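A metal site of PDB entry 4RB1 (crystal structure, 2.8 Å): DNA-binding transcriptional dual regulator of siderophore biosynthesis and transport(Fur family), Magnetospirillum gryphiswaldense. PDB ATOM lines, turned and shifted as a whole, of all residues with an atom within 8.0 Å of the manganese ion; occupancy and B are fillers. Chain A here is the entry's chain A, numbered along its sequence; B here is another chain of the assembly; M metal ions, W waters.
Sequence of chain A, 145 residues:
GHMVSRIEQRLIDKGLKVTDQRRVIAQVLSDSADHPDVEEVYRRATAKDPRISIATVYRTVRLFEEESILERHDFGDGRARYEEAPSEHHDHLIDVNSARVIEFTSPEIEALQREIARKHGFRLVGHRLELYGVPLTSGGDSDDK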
ATOM      1  N   HIS A  89      13.397  16.999   5.021  1.00  0.00           N
ATOM      2  CA  HIS A  89      14.136  18.257   5.076  1.00  0.00           C
ATOM      3  C   HIS A  89      15.627  18.000   5.007  1.00  0.00           C
ATOM      4  O   HIS A  89      16.111  16.973   5.507  1.00  0.00           O
ATOM      5  CB  HIS A  89      13.772  19.029   6.340  1.00  0.00           C
ATOM      6  CG  HIS A  89      14.652  20.228   6.594  1.00  0.00           C
ATOM      7  ND1 HIS A  89      14.414  21.432   6.060  1.00  0.00           N
ATOM      8  CD2 HIS A  89      15.823  20.346   7.338  1.00  0.00           C
ATOM      9  CE1 HIS A  89      15.374  22.290   6.448  1.00  0.00           C
ATOM     10  NE2 HIS A  89      16.229  21.619   7.237  1.00  0.00           N
ATOM     11  N   HIS A  90      16.366  18.894   4.363  1.00  0.00           N
ATOM     12  CA  HIS A  90      17.829  18.880   4.414  1.00  0.00           C
ATOM     13  C   HIS A  90      18.404  20.261   4.372  1.00  0.00           C
ATOM     14  O   HIS A  90      17.848  21.182   3.729  1.00  0.00           O
ATOM     15  CB  HIS A  90      18.435  17.996   3.325  1.00  0.00           C
ATOM     16  CG  HIS A  90      18.303  18.564   1.947  1.00  0.00           C
ATOM     17  ND1 HIS A  90      17.284  18.264   1.137  1.00  0.00           N
ATOM     18  CD2 HIS A  90      19.098  19.475   1.252  1.00  0.00           C
ATOM     19  CE1 HIS A  90      17.418  18.928  -0.022  1.00  0.00           C
ATOM     20  NE2 HIS A  90      18.530  19.675   0.044  1.00  0.00           N
ATOM     21  N   ASP A  91      19.519  20.432   5.073  1.00  0.00           N
ATOM     22  CA  ASP A  91      20.269  21.669   5.083  1.00  0.00           C
ATOM     23  C   ASP A  91      21.458  21.510   4.160  1.00  0.00           C
ATOM     24  O   ASP A  91      21.631  20.462   3.529  1.00  0.00           O
ATOM     25  CB  ASP A  91      20.721  21.979   6.501  1.00  0.00           C
ATOM     26  CG  ASP A  91      19.566  22.016   7.461  1.00  0.00           C
ATOM     27  OD1 ASP A  91      18.733  22.951   7.333  1.00  0.00           O
ATOM     28  OD2 ASP A  91      19.466  21.103   8.334  1.00  0.00           O
ATOM     29  N   HIS A  92      22.281  22.555   4.066  1.00  0.00           N
ATOM     30  CA  HIS A  92      23.351  22.552   3.092  1.00  0.00           C
ATOM     31  C   HIS A  92      24.715  22.875   3.641  1.00  0.00           C
ATOM     32  O   HIS A  92      24.866  23.672   4.577  1.00  0.00           O
ATOM     33  CB  HIS A  92      23.009  23.475   1.930  1.00  0.00           C
ATOM     34  CG  HIS A  92      21.759  23.067   1.194  1.00  0.00           C
ATOM     35  ND1 HIS A  92      20.520  23.387   1.621  1.00  0.00           N
ATOM     36  CD2 HIS A  92      21.593  22.331   0.018  1.00  0.00           C
ATOM     37  CE1 HIS A  92      19.617  22.884   0.765  1.00  0.00           C
ATOM     38  NE2 HIS A  92      20.276  22.245  -0.220  1.00  0.00           N
ATOM     39  N   PHE A 104      22.566  17.720   3.777  1.00  0.00           N
ATOM     40  CA  PHE A 104      22.742  16.945   4.985  1.00  0.00           C
ATOM     41  C   PHE A 104      21.541  17.101   5.894  1.00  0.00           C
ATOM     42  O   PHE A 104      20.887  18.141   5.911  1.00  0.00           O
ATOM     43  CB  PHE A 104      24.034  17.318   5.719  1.00  0.00           C
ATOM     44  CG  PHE A 104      23.896  18.497   6.626  1.00  0.00           C
ATOM     45  CD1 PHE A 104      23.381  18.347   7.914  1.00  0.00           C
ATOM     46  CD2 PHE A 104      24.284  19.770   6.206  1.00  0.00           C
ATOM     47  CE1 PHE A 104      23.241  19.437   8.761  1.00  0.00           C
ATOM     48  CE2 PHE A 104      24.161  20.864   7.051  1.00  0.00           C
ATOM     49  CZ  PHE A 104      23.642  20.698   8.332  1.00  0.00           C
ATOM     50  N   THR A 105      21.272  16.043   6.647  1.00  0.00           N
ATOM     51  CA  THR A 105      20.181  16.028   7.616  1.00  0.00           C
ATOM     52  C   THR A 105      20.712  15.770   9.027  1.00  0.00           C
ATOM     53  O   THR A 105      21.603  14.942   9.229  1.00  0.00           O
ATOM     54  CB  THR A 105      19.091  14.999   7.201  1.00  0.00           C
ATOM     55  OG1 THR A 105      17.829  15.411   7.737  1.00  0.00           O
ATOM     56  CG2 THR A 105      19.436  13.569   7.663  1.00  0.00           C
ATOM     57  N   SER A 106      20.178  16.513   9.990  1.00  0.00           N
ATOM     58  CA  SER A 106      20.536  16.350  11.397  1.00  0.00           C
ATOM     59  C   SER A 106      19.281  16.458  12.268  1.00  0.00           C
ATOM     60  O   SER A 106      18.756  17.559  12.483  1.00  0.00           O
ATOM     61  CB  SER A 106      21.570  17.397  11.816  1.00  0.00           C
ATOM     62  OG  SER A 106      21.730  17.433  13.220  1.00  0.00           O
ATOM     63  N   ILE A 109      19.463  18.668  15.734  1.00  0.00           N
ATOM     64  CA  ILE A 109      19.536  20.118  15.550  1.00  0.00           C
ATOM     65  C   ILE A 109      18.140  20.757  15.486  1.00  0.00           C
ATOM     66  O   ILE A 109      17.890  21.728  16.198  1.00  0.00           O
ATOM     67  CB  ILE A 109      20.393  20.518  14.316  1.00  0.00           C
ATOM     68  CG1 ILE A 109      21.881  20.491  14.670  1.00  0.00           C
ATOM     69  CG2 ILE A 109      20.022  21.913  13.818  1.00  0.00           C
ATOM     70  CD1 ILE A 109      22.804  20.915  13.548  1.00  0.00           C
ATOM     71  N   GLU A 110      17.260  20.189  14.664  1.00  0.00           N
ATOM     72  CA  GLU A 110      15.882  20.684  14.508  1.00  0.00           C
ATOM     73  C   GLU A 110      15.150  20.738  15.848  1.00  0.00           C
ATOM     74  O   GLU A 110      14.385  21.671  16.117  1.00  0.00           O
ATOM     75  CB  GLU A 110      15.086  19.788  13.560  1.00  0.00           C
ATOM     76  CG  GLU A 110      15.836  19.331  12.326  1.00  0.00           C
ATOM     77  CD  GLU A 110      16.212  20.469  11.397  1.00  0.00           C
ATOM     78  OE1 GLU A 110      15.653  21.575  11.533  1.00  0.00           O
ATOM     79  OE2 GLU A 110      17.072  20.232  10.518  1.00  0.00           O
ATOM     80  N   GLN A 113      16.542  23.472  17.804  1.00  0.00           N
ATOM     81  CA  GLN A 113      15.967  24.650  17.165  1.00  0.00           C
ATOM     82  C   GLN A 113      14.537  24.961  17.612  1.00  0.00           C
ATOM     83  O   GLN A 113      14.187  26.119  17.852  1.00  0.00           O
ATOM     84  CB  GLN A 113      16.051  24.513  15.652  1.00  0.00           C
ATOM     85  CG  GLN A 113      17.483  24.488  15.132  1.00  0.00           C
ATOM     86  CD  GLN A 113      17.581  24.463  13.624  1.00  0.00           C
ATOM     87  OE1 GLN A 113      16.566  24.419  12.919  1.00  0.00           O
ATOM     88  NE2 GLN A 113      18.795  24.496  13.107  1.00  0.00           N
ATOM     89  N   HIS A 127      13.128  27.835   9.228  1.00  0.00           N
ATOM     90  CA  HIS A 127      14.506  28.090   9.619  1.00  0.00           C
ATOM     91  C   HIS A 127      15.368  27.979   8.392  1.00  0.00           C
ATOM     92  O   HIS A 127      14.895  27.576   7.319  1.00  0.00           O
ATOM     93  CB  HIS A 127      14.942  27.050  10.630  1.00  0.00           C
ATOM     94  CG  HIS A 127      15.199  25.702  10.016  1.00  0.00           C
ATOM     95  ND1 HIS A 127      14.225  24.857   9.678  1.00  0.00           N
ATOM     96  CD2 HIS A 127      16.397  25.095   9.629  1.00  0.00           C
ATOM     97  CE1 HIS A 127      14.750  23.752   9.130  1.00  0.00           C
ATOM     98  NE2 HIS A 127      16.079  23.897   9.105  1.00  0.00           N
ATOM     99  N   ARG A 128      16.645  28.315   8.546  1.00  0.00           N
ATOM    100  CA  ARG A 128      17.618  28.202   7.465  1.00  0.00           C
ATOM    101  C   ARG A 128      19.003  27.961   8.071  1.00  0.00           C
ATOM    102  O   ARG A 128      19.446  28.727   8.922  1.00  0.00           O
ATOM    103  CB  ARG A 128      17.589  29.465   6.619  1.00  0.00           C
ATOM    104  CG  ARG A 128      18.838  29.718   5.786  1.00  0.00           C
ATOM    105  CD  ARG A 128      18.730  31.041   5.035  1.00  0.00           C
ATOM    106  NE  ARG A 128      19.948  31.833   5.174  1.00  0.00           N
ATOM    107  CZ  ARG A 128      20.446  32.634   4.235  1.00  0.00           C
ATOM    108  NH1 ARG A 128      19.850  32.743   3.043  1.00  0.00           N
ATOM    109  NH2 ARG A 128      21.548  33.320   4.482  1.00  0.00           N
ATOM    110  N   LEU A 129      19.648  26.884   7.641  1.00  0.00           N
ATOM    111  CA  LEU A 129      20.991  26.558   8.100  1.00  0.00           C
ATOM    112  C   LEU A 129      21.871  26.200   6.922  1.00  0.00           C
ATOM    113  O   LEU A 129      21.586  25.260   6.183  1.00  0.00           O
ATOM    114  CB  LEU A 129      20.976  25.407   9.108  1.00  0.00           C
ATOM    115  CG  LEU A 129      22.339  24.877   9.605  1.00  0.00           C
ATOM    116  CD1 LEU A 129      23.034  25.839  10.560  1.00  0.00           C
ATOM    117  CD2 LEU A 129      22.238  23.502  10.252  1.00  0.00           C
ATOM    118  N   GLU A 130      22.943  26.973   6.736  1.00  0.00           N
ATOM    119  CA  GLU A 130      23.948  26.667   5.719  1.00  0.00           C
ATOM    120  C   GLU A 130      25.323  26.814   6.321  1.00  0.00           C
ATOM    121  O   GLU A 130      25.572  27.726   7.110  1.00  0.00           O
ATOM    122  CB  GLU A 130      23.781  27.521   4.461  1.00  0.00           C
ATOM    123  CG  GLU A 130      23.373  28.944   4.749  1.00  0.00           C
ATOM    124  CD  GLU A 130      22.294  29.464   3.810  1.00  0.00           C
ATOM    125  OE1 GLU A 130      22.497  30.581   3.261  1.00  0.00           O
ATOM    126  OE2 GLU A 130      21.266  28.765   3.622  1.00  0.00           O
ATOM    127  N   LEU B 129      22.979  30.456  10.295  1.00  0.00           N
ATOM    128  CA  LEU B 129      21.819  29.823  10.901  1.00  0.00           C
ATOM    129  C   LEU B 129      20.825  30.857  11.413  1.00  0.00           C
ATOM    130  O   LEU B 129      21.117  31.603  12.359  1.00  0.00           O
ATOM    131  CB  LEU B 129      22.200  28.878  12.061  1.00  0.00           C
ATOM    132  CG  LEU B 129      20.965  28.491  12.895  1.00  0.00           C
ATOM    133  CD1 LEU B 129      20.108  27.462  12.174  1.00  0.00           C
ATOM    134  CD2 LEU B 129      21.271  28.060  14.322  1.00  0.00           C
ATOM    135  N   GLU B 130      19.648  30.879  10.807  1.00  0.00           N
ATOM    136  CA  GLU B 130      18.582  31.779  11.193  1.00  0.00           C
ATOM    137  C   GLU B 130      17.306  31.012  11.473  1.00  0.00           C
ATOM    138  O   GLU B 130      16.964  30.076  10.757  1.00  0.00           O
ATOM    139  CB  GLU B 130      18.319  32.800  10.104  1.00  0.00           C
ATOM    140  CG  GLU B 130      19.522  33.636   9.713  1.00  0.00           C
ATOM    141  CD  GLU B 130      19.417  34.172   8.306  1.00  0.00           C
ATOM    142  OE1 GLU B 130      20.286  34.993   7.911  1.00  0.00           O
ATOM    143  OE2 GLU B 130      18.452  33.771   7.602  1.00  0.00           O
ATOM    144  N   LEU B 131      16.632  31.434  12.529  1.00  0.00           N
ATOM    145  CA  LEU B 131      15.336  30.911  12.896  1.00  0.00           C
ATOM    146  C   LEU B 131      14.251  31.952  12.657  1.00  0.00           C
ATOM    147  O   LEU B 131      14.435  33.124  12.994  1.00  0.00           O
ATOM    148  CB  LEU B 131      15.368  30.514  14.365  1.00  0.00           C
ATOM    149  CG  LEU B 131      15.811  29.084  14.702  1.00  0.00           C
ATOM    150  CD1 LEU B 131      16.971  28.591  13.857  1.00  0.00           C
ATOM    151  CD2 LEU B 131      16.136  29.011  16.185  1.00  0.00           C
HETATM  152 MN    MN M   1      17.379  22.406   9.063  1.00  0.00          MN
HETATM  153  O   HOH W   1      18.681  22.675  10.718  1.00  0.00           O
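Water W1 bridges NE2 of Gln 113 (3.0 Å) and OE1 of Glu 110 (3.3 Å).
The backbone carbonyl oxygen of His 89 lies within hydrogen-bond range of the side-chain hydroxyl of Thr 105 (3.2 Å).
The side-chain carboxylate of Glu 110 lies close to the side-chain amide oxygen of Gln 113 (3.3 Å).
The backbone NH (N) of Asp 91 lies within hydrogen-bond range of the backbone carbonyl oxygen (O) of Phe 104 (2.8 Å).
The manganese ion is bound by NE2 of His 127 (2.0 Å), water W1 (2.1 Å), OD1 of Asp 91 (2.3 Å), NE2 of His 89 (2.3 Å), OD2 of Asp 91 (2.6 Å) and OE2 of Glu 110 (2.6 Å).
Four residues have an atom within 4 Å of the manganese ion: His 89, Asp 91, Glu 110 and His 127.
The nearest printed residue that does not touch the manganese ion is Gln 113 (4.4 Å).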
